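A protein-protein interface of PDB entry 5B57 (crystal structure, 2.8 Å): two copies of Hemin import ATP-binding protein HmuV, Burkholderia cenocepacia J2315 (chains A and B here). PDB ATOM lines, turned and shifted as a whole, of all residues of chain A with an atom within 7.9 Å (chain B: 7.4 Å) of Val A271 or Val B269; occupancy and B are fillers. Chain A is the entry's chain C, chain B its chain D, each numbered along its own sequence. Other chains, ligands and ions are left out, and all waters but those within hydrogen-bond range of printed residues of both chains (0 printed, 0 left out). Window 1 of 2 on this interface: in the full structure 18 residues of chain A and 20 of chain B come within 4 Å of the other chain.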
ATOM      1  N   ASN A 217       0.131   1.720 -20.933  1.00  0.00           N
ATOM      2  CA  ASN A 217       0.877   1.863 -22.178  1.00  0.00           C
ATOM      3  C   ASN A 217       0.245   2.903 -23.097  1.00  0.00           C
ATOM      4  O   ASN A 217       0.956   3.594 -23.841  1.00  0.00           O
ATOM      5  CB  ASN A 217       0.984   0.518 -22.878  1.00  0.00           C
ATOM      6  CG  ASN A 217       2.029  -0.360 -22.260  1.00  0.00           C
ATOM      7  OD1 ASN A 217       2.994   0.133 -21.682  1.00  0.00           O
ATOM      8  ND2 ASN A 217       1.852  -1.668 -22.378  1.00  0.00           N
ATOM      9  N   PRO A 246       9.086   0.252 -12.923  1.00  0.00           N
ATOM     10  CA  PRO A 246       8.513  -0.899 -12.220  1.00  0.00           C
ATOM     11  C   PRO A 246       8.073  -0.590 -10.805  1.00  0.00           C
ATOM     12  O   PRO A 246       7.006  -1.059 -10.382  1.00  0.00           O
ATOM     13  CB  PRO A 246       9.650  -1.915 -12.272  1.00  0.00           C
ATOM     14  CG  PRO A 246      10.303  -1.617 -13.546  1.00  0.00           C
ATOM     15  CD  PRO A 246      10.323  -0.121 -13.618  1.00  0.00           C
ATOM     16  N   ILE A 249       4.577   1.647 -11.123  1.00  0.00           N
ATOM     17  CA  ILE A 249       3.524   0.709 -11.468  1.00  0.00           C
ATOM     18  C   ILE A 249       3.256  -0.236 -10.313  1.00  0.00           C
ATOM     19  O   ILE A 249       2.107  -0.628 -10.078  1.00  0.00           O
ATOM     20  CB  ILE A 249       3.905  -0.043 -12.755  1.00  0.00           C
ATOM     21  CG1 ILE A 249       3.994   0.963 -13.889  1.00  0.00           C
ATOM     22  CG2 ILE A 249       2.865  -1.094 -13.107  1.00  0.00           C
ATOM     23  CD1 ILE A 249       2.764   1.795 -13.989  1.00  0.00           C
ATOM     24  N   PHE A 255       0.947  -4.308  -9.168  1.00  0.00           N
ATOM     25  CA  PHE A 255       1.126  -5.173 -10.330  1.00  0.00           C
ATOM     26  C   PHE A 255       2.612  -5.194 -10.697  1.00  0.00           C
ATOM     27  O   PHE A 255       3.180  -4.163 -11.075  1.00  0.00           O
ATOM     28  CB  PHE A 255       0.255  -4.680 -11.491  1.00  0.00           C
ATOM     29  CG  PHE A 255       0.332  -5.538 -12.721  1.00  0.00           C
ATOM     30  CD1 PHE A 255       0.385  -6.925 -12.616  1.00  0.00           C
ATOM     31  CD2 PHE A 255       0.335  -4.959 -13.987  1.00  0.00           C
ATOM     32  CE1 PHE A 255       0.459  -7.715 -13.751  1.00  0.00           C
ATOM     33  CE2 PHE A 255       0.413  -5.747 -15.127  1.00  0.00           C
ATOM     34  CZ  PHE A 255       0.476  -7.123 -15.005  1.00  0.00           C
ATOM     35  N   ALA A 256       3.238  -6.367 -10.586  1.00  0.00           N
ATOM     36  CA  ALA A 256       4.678  -6.498 -10.787  1.00  0.00           C
ATOM     37  C   ALA A 256       5.006  -6.489 -12.280  1.00  0.00           C
ATOM     38  O   ALA A 256       4.734  -7.471 -12.980  1.00  0.00           O
ATOM     39  CB  ALA A 256       5.175  -7.780 -10.125  1.00  0.00           C
ATOM     40  N   VAL A 257       5.592  -5.394 -12.778  1.00  0.00           N
ATOM     41  CA  VAL A 257       5.854  -5.285 -14.216  1.00  0.00           C
ATOM     42  C   VAL A 257       7.331  -5.062 -14.498  1.00  0.00           C
ATOM     43  O   VAL A 257       8.147  -4.944 -13.582  1.00  0.00           O
ATOM     44  CB  VAL A 257       5.062  -4.139 -14.877  1.00  0.00           C
ATOM     45  CG1 VAL A 257       3.535  -4.229 -14.599  1.00  0.00           C
ATOM     46  CG2 VAL A 257       5.668  -2.809 -14.454  1.00  0.00           C
ATOM     47  N   LYS A 258       7.673  -4.972 -15.775  1.00  0.00           N
ATOM     48  CA  LYS A 258       8.970  -4.489 -16.210  1.00  0.00           C
ATOM     49  C   LYS A 258       8.769  -3.640 -17.453  1.00  0.00           C
ATOM     50  O   LYS A 258       7.758  -3.752 -18.149  1.00  0.00           O
ATOM     51  CB  LYS A 258       9.926  -5.636 -16.517  1.00  0.00           C
ATOM     52  CG  LYS A 258       9.507  -6.482 -17.713  1.00  0.00           C
ATOM     53  CD  LYS A 258      10.679  -7.319 -18.208  1.00  0.00           C
ATOM     54  CE  LYS A 258      10.252  -8.427 -19.156  1.00  0.00           C
ATOM     55  NZ  LYS A 258       9.587  -9.557 -18.449  1.00  0.00           N
ATOM     56  N   MET A 259       9.737  -2.778 -17.727  1.00  0.00           N
ATOM     57  CA  MET A 259       9.692  -1.934 -18.914  1.00  0.00           C
ATOM     58  C   MET A 259      10.513  -2.565 -20.041  1.00  0.00           C
ATOM     59  O   MET A 259      11.387  -3.399 -19.810  1.00  0.00           O
ATOM     60  CB  MET A 259      10.191  -0.522 -18.580  1.00  0.00           C
ATOM     61  CG  MET A 259       9.298   0.213 -17.570  1.00  0.00           C
ATOM     62  SD  MET A 259       7.567   0.352 -18.087  1.00  0.00           S
ATOM     63  CE  MET A 259       6.797   0.523 -16.484  1.00  0.00           C
ATOM     64  N   VAL A 260      10.190  -2.190 -21.277  1.00  0.00           N
ATOM     65  CA  VAL A 260      10.831  -2.733 -22.476  1.00  0.00           C
ATOM     66  C   VAL A 260      10.884  -1.623 -23.521  1.00  0.00           C
ATOM     67  O   VAL A 260       9.957  -0.811 -23.618  1.00  0.00           O
ATOM     68  CB  VAL A 260      10.065  -3.968 -23.006  1.00  0.00           C
ATOM     69  CG1 VAL A 260      10.546  -4.351 -24.379  1.00  0.00           C
ATOM     70  CG2 VAL A 260      10.194  -5.148 -22.066  1.00  0.00           C
ATOM     71  N   GLU A 261      11.956  -1.595 -24.319  1.00  0.00           N
ATOM     72  CA  GLU A 261      12.212  -0.499 -25.255  1.00  0.00           C
ATOM     73  C   GLU A 261      11.598  -0.747 -26.643  1.00  0.00           C
ATOM     74  O   GLU A 261      11.171  -1.851 -26.977  1.00  0.00           O
ATOM     75  CB  GLU A 261      13.719  -0.273 -25.392  1.00  0.00           C
ATOM     76  CG  GLU A 261      14.392   0.311 -24.159  1.00  0.00           C
ATOM     77  CD  GLU A 261      14.150   1.801 -24.001  1.00  0.00           C
ATOM     78  OE1 GLU A 261      13.924   2.501 -25.021  1.00  0.00           O
ATOM     79  OE2 GLU A 261      14.186   2.273 -22.845  1.00  0.00           O
ATOM     80  N   THR A 262      11.548   0.315 -27.454  1.00  0.00           N
ATOM     81  CA  THR A 262      11.208   0.227 -28.884  1.00  0.00           C
ATOM     82  C   THR A 262      12.214   1.077 -29.676  1.00  0.00           C
ATOM     83  O   THR A 262      13.244   1.520 -29.151  1.00  0.00           O
ATOM     84  CB  THR A 262       9.744   0.634 -29.154  1.00  0.00           C
ATOM     85  OG1 THR A 262       9.516   2.019 -28.823  1.00  0.00           O
ATOM     86  CG2 THR A 262       8.775  -0.270 -28.369  1.00  0.00           C
ATOM     87  N   PRO A 268       8.631   3.842 -23.997  1.00  0.00           N
ATOM     88  CA  PRO A 268       8.866   2.467 -23.524  1.00  0.00           C
ATOM     89  C   PRO A 268       7.610   1.807 -22.961  1.00  0.00           C
ATOM     90  O   PRO A 268       6.793   2.486 -22.330  1.00  0.00           O
ATOM     91  CB  PRO A 268       9.928   2.668 -22.435  1.00  0.00           C
ATOM     92  CG  PRO A 268       9.590   4.024 -21.843  1.00  0.00           C
ATOM     93  CD  PRO A 268       8.889   4.840 -22.944  1.00  0.00           C
ATOM     94  N   VAL A 269       7.447   0.480 -23.172  1.00  0.00           N
ATOM     95  CA  VAL A 269       6.187  -0.223 -22.889  1.00  0.00           C
ATOM     96  C   VAL A 269       6.297  -1.046 -21.615  1.00  0.00           C
ATOM     97  O   VAL A 269       7.317  -1.696 -21.354  1.00  0.00           O
ATOM     98  CB  VAL A 269       5.723  -1.137 -24.047  1.00  0.00           C
ATOM     99  CG1 VAL A 269       4.995  -0.334 -25.126  1.00  0.00           C
ATOM    100  CG2 VAL A 269       6.878  -1.986 -24.596  1.00  0.00           C
ATOM    101  N   MET A 270       5.211  -1.041 -20.845  1.00  0.00           N
ATOM    102  CA  MET A 270       5.083  -1.864 -19.658  1.00  0.00           C
ATOM    103  C   MET A 270       4.620  -3.247 -20.056  1.00  0.00           C
ATOM    104  O   MET A 270       3.744  -3.407 -20.912  1.00  0.00           O
ATOM    105  CB  MET A 270       4.081  -1.247 -18.687  1.00  0.00           C
ATOM    106  CG  MET A 270       3.710  -2.111 -17.478  1.00  0.00           C
ATOM    107  SD  MET A 270       2.250  -1.437 -16.680  1.00  0.00           S
ATOM    108  CE  MET A 270       2.665   0.259 -16.997  1.00  0.00           C
ATOM    109  N   VAL A 271       5.185  -4.242 -19.383  1.00  0.00           N
ATOM    110  CA  VAL A 271       5.020  -5.657 -19.690  1.00  0.00           C
ATOM    111  C   VAL A 271       5.039  -6.382 -18.347  1.00  0.00           C
ATOM    112  O   VAL A 271       5.741  -5.939 -17.425  1.00  0.00           O
ATOM    113  CB  VAL A 271       6.120  -6.102 -20.676  1.00  0.00           C
ATOM    114  CG1 VAL A 271       6.520  -7.570 -20.506  1.00  0.00           C
ATOM    115  CG2 VAL A 271       5.694  -5.776 -22.111  1.00  0.00           C
ATOM    116  N   PRO A 272       4.258  -7.447 -18.159  1.00  0.00           N
ATOM    117  CA  PRO A 272       4.222  -8.141 -16.863  1.00  0.00           C
ATOM    118  C   PRO A 272       5.445  -9.046 -16.685  1.00  0.00           C
ATOM    119  O   PRO A 272       6.308  -9.130 -17.562  1.00  0.00           O
ATOM    120  CB  PRO A 272       2.925  -8.952 -16.940  1.00  0.00           C
ATOM    121  CG  PRO A 272       2.176  -8.427 -18.165  1.00  0.00           C
ATOM    122  CD  PRO A 272       3.251  -7.974 -19.094  1.00  0.00           C
ATOM    123  N   ALA A 273       5.494  -9.733 -15.527  1.00  0.00           N
ATOM    124  CA  ALA A 273       6.571 -10.681 -15.085  1.00  0.00           C
ATOM    125  C   ALA A 273       7.926 -10.026 -14.886  1.00  0.00           C
ATOM    126  O   ALA A 273       7.995  -8.874 -14.480  1.00  0.00           O
ATOM    127  CB  ALA A 273       6.732 -11.852 -16.049  1.00  0.00           C
ATOM    128  N   HIS B 192      -5.038 -10.139 -14.941  1.00  0.00           N
ATOM    129  CA  HIS B 192      -3.982 -11.128 -15.175  1.00  0.00           C
ATOM    130  C   HIS B 192      -4.161 -12.361 -14.297  1.00  0.00           C
ATOM    131  O   HIS B 192      -4.055 -13.494 -14.778  1.00  0.00           O
ATOM    132  CB  HIS B 192      -2.622 -10.499 -14.929  1.00  0.00           C
ATOM    133  CG  HIS B 192      -2.074  -9.766 -16.111  1.00  0.00           C
ATOM    134  ND1 HIS B 192      -1.549 -10.416 -17.206  1.00  0.00           N
ATOM    135  CD2 HIS B 192      -1.959  -8.441 -16.364  1.00  0.00           C
ATOM    136  CE1 HIS B 192      -1.132  -9.522 -18.083  1.00  0.00           C
ATOM    137  NE2 HIS B 192      -1.367  -8.315 -17.596  1.00  0.00           N
ATOM    138  N   ASN B 217      -2.542  -8.186 -26.238  1.00  0.00           N
ATOM    139  CA  ASN B 217      -1.428  -8.654 -25.433  1.00  0.00           C
ATOM    140  C   ASN B 217      -1.886  -9.482 -24.232  1.00  0.00           C
ATOM    141  O   ASN B 217      -1.150 -10.363 -23.763  1.00  0.00           O
ATOM    142  CB  ASN B 217      -0.609  -7.452 -24.997  1.00  0.00           C
ATOM    143  CG  ASN B 217       0.088  -6.805 -26.150  1.00  0.00           C
ATOM    144  OD1 ASN B 217       0.631  -7.495 -27.023  1.00  0.00           O
ATOM    145  ND2 ASN B 217       0.078  -5.478 -26.181  1.00  0.00           N
ATOM    146  N   ALA B 220      -2.332 -12.943 -25.754  1.00  0.00           N
ATOM    147  CA  ALA B 220      -0.984 -13.462 -25.997  1.00  0.00           C
ATOM    148  C   ALA B 220      -0.403 -14.137 -24.758  1.00  0.00           C
ATOM    149  O   ALA B 220       0.160 -15.248 -24.828  1.00  0.00           O
ATOM    150  CB  ALA B 220      -0.063 -12.318 -26.421  1.00  0.00           C
ATOM    151  N   ARG B 221      -0.501 -13.449 -23.616  1.00  0.00           N
ATOM    152  CA  ARG B 221       0.144 -13.896 -22.404  1.00  0.00           C
ATOM    153  C   ARG B 221      -0.616 -15.017 -21.700  1.00  0.00           C
ATOM    154  O   ARG B 221      -0.013 -15.736 -20.895  1.00  0.00           O
ATOM    155  CB  ARG B 221       0.332 -12.709 -21.480  1.00  0.00           C
ATOM    156  CG  ARG B 221       1.256 -13.012 -20.365  1.00  0.00           C
ATOM    157  CD  ARG B 221       1.371 -11.833 -19.475  1.00  0.00           C
ATOM    158  NE  ARG B 221       2.046 -12.204 -18.239  1.00  0.00           N
ATOM    159  CZ  ARG B 221       3.367 -12.275 -18.102  1.00  0.00           C
ATOM    160  NH1 ARG B 221       3.868 -12.630 -16.924  1.00  0.00           N
ATOM    161  NH2 ARG B 221       4.178 -11.996 -19.131  1.00  0.00           N
ATOM    162  N   MET B 244       0.135 -13.719 -33.896  1.00  0.00           N
ATOM    163  CA  MET B 244       0.384 -12.335 -33.524  1.00  0.00           C
ATOM    164  C   MET B 244       1.354 -11.637 -34.476  1.00  0.00           C
ATOM    165  O   MET B 244       2.465 -11.285 -34.076  1.00  0.00           O
ATOM    166  CB  MET B 244       0.930 -12.283 -32.101  1.00  0.00           C
ATOM    167  CG  MET B 244       0.527 -11.045 -31.348  1.00  0.00           C
ATOM    168  SD  MET B 244      -1.158 -11.218 -30.772  1.00  0.00           S
ATOM    169  CE  MET B 244      -0.843 -12.604 -29.720  1.00  0.00           C
ATOM    170  N   VAL B 257       0.687  -2.305 -36.515  1.00  0.00           N
ATOM    171  CA  VAL B 257       1.495  -2.546 -35.329  1.00  0.00           C
ATOM    172  C   VAL B 257       2.794  -3.234 -35.708  1.00  0.00           C
ATOM    173  O   VAL B 257       2.993  -3.676 -36.839  1.00  0.00           O
ATOM    174  CB  VAL B 257       0.776  -3.399 -34.265  1.00  0.00           C
ATOM    175  CG1 VAL B 257      -0.555  -2.750 -33.798  1.00  0.00           C
ATOM    176  CG2 VAL B 257       0.612  -4.835 -34.782  1.00  0.00           C
ATOM    177  N   LYS B 258       3.671  -3.341 -34.715  1.00  0.00           N
ATOM    178  CA  LYS B 258       4.886  -4.131 -34.779  1.00  0.00           C
ATOM    179  C   LYS B 258       5.007  -4.945 -33.498  1.00  0.00           C
ATOM    180  O   LYS B 258       4.300  -4.709 -32.516  1.00  0.00           O
ATOM    181  CB  LYS B 258       6.123  -3.244 -34.969  1.00  0.00           C
ATOM    182  CG  LYS B 258       6.535  -2.395 -33.756  1.00  0.00           C
ATOM    183  CD  LYS B 258       7.734  -1.520 -34.124  1.00  0.00           C
ATOM    184  CE  LYS B 258       7.956  -0.372 -33.154  1.00  0.00           C
ATOM    185  NZ  LYS B 258       8.473  -0.838 -31.850  1.00  0.00           N
ATOM    186  N   MET B 259       5.916  -5.914 -33.507  1.00  0.00           N
ATOM    187  CA  MET B 259       6.100  -6.795 -32.367  1.00  0.00           C
ATOM    188  C   MET B 259       7.509  -6.636 -31.814  1.00  0.00           C
ATOM    189  O   MET B 259       8.470  -6.482 -32.570  1.00  0.00           O
ATOM    190  CB  MET B 259       5.839  -8.267 -32.740  1.00  0.00           C
ATOM    191  CG  MET B 259       4.496  -8.569 -33.439  1.00  0.00           C
ATOM    192  SD  MET B 259       2.986  -8.282 -32.469  1.00  0.00           S
ATOM    193  CE  MET B 259       3.428  -8.987 -30.887  1.00  0.00           C
ATOM    194  N   VAL B 260       7.611  -6.691 -30.486  1.00  0.00           N
ATOM    195  CA  VAL B 260       8.830  -6.526 -29.705  1.00  0.00           C
ATOM    196  C   VAL B 260       8.977  -7.729 -28.772  1.00  0.00           C
ATOM    197  O   VAL B 260       7.986  -8.300 -28.300  1.00  0.00           O
ATOM    198  CB  VAL B 260       8.792  -5.195 -28.902  1.00  0.00           C
ATOM    199  CG1 VAL B 260       9.958  -5.101 -27.932  1.00  0.00           C
ATOM    200  CG2 VAL B 260       8.726  -3.965 -29.848  1.00  0.00           C
ATOM    201  N   GLU B 261      10.224  -8.122 -28.500  1.00  0.00           N
ATOM    202  CA  GLU B 261      10.477  -9.339 -27.739  1.00  0.00           C
ATOM    203  C   GLU B 261      10.499  -9.048 -26.240  1.00  0.00           C
ATOM    204  O   GLU B 261      10.340  -7.903 -25.804  1.00  0.00           O
ATOM    205  CB  GLU B 261      11.783  -9.985 -28.200  1.00  0.00           C
ATOM    206  CG  GLU B 261      11.901 -10.118 -29.723  1.00  0.00           C
ATOM    207  CD  GLU B 261      11.183 -11.330 -30.305  1.00  0.00           C
ATOM    208  OE1 GLU B 261      11.194 -11.451 -31.548  1.00  0.00           O
ATOM    209  OE2 GLU B 261      10.626 -12.157 -29.547  1.00  0.00           O
ATOM    210  N   THR B 262      10.696 -10.093 -25.437  1.00  0.00           N
ATOM    211  CA  THR B 262      10.675  -9.945 -23.989  1.00  0.00           C
ATOM    212  C   THR B 262      11.642 -10.936 -23.329  1.00  0.00           C
ATOM    213  O   THR B 262      12.173 -10.671 -22.247  1.00  0.00           O
ATOM    214  CB  THR B 262       9.237 -10.136 -23.490  1.00  0.00           C
ATOM    215  OG1 THR B 262       8.475  -8.989 -23.886  1.00  0.00           O
ATOM    216  CG2 THR B 262       9.150 -10.307 -21.987  1.00  0.00           C
ATOM    217  N   PRO B 267       6.295 -14.731 -25.324  1.00  0.00           N
ATOM    218  CA  PRO B 267       5.352 -13.620 -25.144  1.00  0.00           C
ATOM    219  C   PRO B 267       5.836 -12.289 -25.745  1.00  0.00           C
ATOM    220  O   PRO B 267       6.188 -11.381 -24.988  1.00  0.00           O
ATOM    221  CB  PRO B 267       5.247 -13.507 -23.623  1.00  0.00           C
ATOM    222  CG  PRO B 267       6.606 -13.959 -23.140  1.00  0.00           C
ATOM    223  CD  PRO B 267       6.990 -15.082 -24.070  1.00  0.00           C
ATOM    224  N   PRO B 268       5.846 -12.167 -27.077  1.00  0.00           N
ATOM    225  CA  PRO B 268       6.223 -10.887 -27.704  1.00  0.00           C
ATOM    226  C   PRO B 268       5.033  -9.936 -27.726  1.00  0.00           C
ATOM    227  O   PRO B 268       3.919 -10.337 -28.068  1.00  0.00           O
ATOM    228  CB  PRO B 268       6.637 -11.300 -29.122  1.00  0.00           C
ATOM    229  CG  PRO B 268       5.781 -12.510 -29.412  1.00  0.00           C
ATOM    230  CD  PRO B 268       5.537 -13.210 -28.079  1.00  0.00           C
ATOM    231  N   VAL B 269       5.263  -8.656 -27.357  1.00  0.00           N
ATOM    232  CA  VAL B 269       4.159  -7.727 -27.115  1.00  0.00           C
ATOM    233  C   VAL B 269       3.947  -6.811 -28.317  1.00  0.00           C
ATOM    234  O   VAL B 269       4.880  -6.414 -29.016  1.00  0.00           O
ATOM    235  CB  VAL B 269       4.358  -6.899 -25.822  1.00  0.00           C
ATOM    236  CG1 VAL B 269       4.230  -7.792 -24.590  1.00  0.00           C
ATOM    237  CG2 VAL B 269       5.686  -6.163 -25.845  1.00  0.00           C
ATOM    238  N   MET B 270       2.681  -6.467 -28.537  1.00  0.00           N
ATOM    239  CA  MET B 270       2.236  -5.672 -29.667  1.00  0.00           C
ATOM    240  C   MET B 270       2.340  -4.193 -29.327  1.00  0.00           C
ATOM    241  O   MET B 270       2.031  -3.781 -28.207  1.00  0.00           O
ATOM    242  CB  MET B 270       0.789  -6.045 -30.002  1.00  0.00           C
ATOM    243  CG  MET B 270       0.160  -5.393 -31.215  1.00  0.00           C
ATOM    244  SD  MET B 270      -1.629  -5.738 -31.200  1.00  0.00           S
ATOM    245  CE  MET B 270      -2.192  -4.764 -29.790  1.00  0.00           C
ATOM    246  N   VAL B 271       2.770  -3.398 -30.300  1.00  0.00           N
ATOM    247  CA  VAL B 271       3.043  -1.971 -30.125  1.00  0.00           C
ATOM    248  C   VAL B 271       2.727  -1.306 -31.455  1.00  0.00           C
ATOM    249  O   VAL B 271       2.935  -1.907 -32.513  1.00  0.00           O
ATOM    250  CB  VAL B 271       4.520  -1.719 -29.712  1.00  0.00           C
ATOM    251  CG1 VAL B 271       4.974  -0.285 -30.016  1.00  0.00           C
ATOM    252  CG2 VAL B 271       4.728  -2.040 -28.246  1.00  0.00           C
ATOM    253  N   PRO B 272       2.203  -0.081 -31.450  1.00  0.00           N
ATOM    254  CA  PRO B 272       1.926   0.599 -32.726  1.00  0.00           C
ATOM    255  C   PRO B 272       3.200   1.021 -33.453  1.00  0.00           C
ATOM    256  O   PRO B 272       4.253   0.424 -33.232  1.00  0.00           O
ATOM    257  CB  PRO B 272       1.082   1.807 -32.313  1.00  0.00           C
ATOM    258  CG  PRO B 272       0.541   1.449 -30.937  1.00  0.00           C
ATOM    259  CD  PRO B 272       1.648   0.658 -30.305  1.00  0.00           C
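The backbone NH (N) of Ala A273 lies within hydrogen-bond range of the backbone carbonyl oxygen (O) of Ala A256 (3.5 Å).
The backbone NH of Lys A258 sits at hydrogen-bond distance from the backbone carbonyl oxygen of Val A271.
NZ of Lys A258 is in hydrogen-bond range of O of Pro A272 (3.4 Å).
The backbone carbonyl oxygen (O) of Val A260 sits at hydrogen-bond distance from the backbone NH (N) of Val A269 (2.9 Å).
N of Lys B258 sits at hydrogen-bond distance from O of Val B271.
The side-chain hydroxyl of Thr B262 sits at hydrogen-bond distance from the backbone carbonyl oxygen of Pro B267, at 3.5 Å.
His B192 touches Phe A255 (CD2 to CZ, 3.1 Å).
CG2 of Thr B262 touches CE of Lys A258, 3.6 Å away.
Val B260 touches Val A260.
Val A260 touches Glu B261.
Glu A261 touches Val B260.
Thr A262 touches Lys B258 (CB to NZ, 3.3 Å).
Thr A262 touches Val B260.
Val A271 touches Val B269 (CG2 to CG1, 3.5 Å).
Pro A272 touches Arg B221.
Ala A273 touches Arg B221.
Of chain A, only Val A271 comes within 4 Å of Val B269.
Of the printed residues of chain B, Val A260 touches Val B260 (3.7 Å) and Glu B261 (3.8 Å).
Of the printed residues of chain A, Glu B261 touches Val A260.
Of the 17 printed residues of chain A, 9 touch a printed residue of chain B.
Of the 17 printed residues of chain B, 8 touch a printed residue of chain A.
Printed residues of chain B that touch a printed residue of chain A: His B192, Arg B221, Lys B258, Val B260, Glu B261, Thr B262, Val B269 and Val B271.
Among the printed residues, 12 pairs touch across the chains.
Among the printed residues, no Asp or Glu carboxylate lies within 4 Å of a Lys or Arg side-chain nitrogen of the other chain.
Lys A258 touches Thr B262, and with the chains exchanged Thr A262 touches Lys B258.
Val A260 touches its own counterpart, Val B260.
Val A260 touches Glu B261, and with the chains exchanged Glu A261 touches Val B260.
Val A269 touches Val B271, and with the chains exchanged Val A271 touches Val B269.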
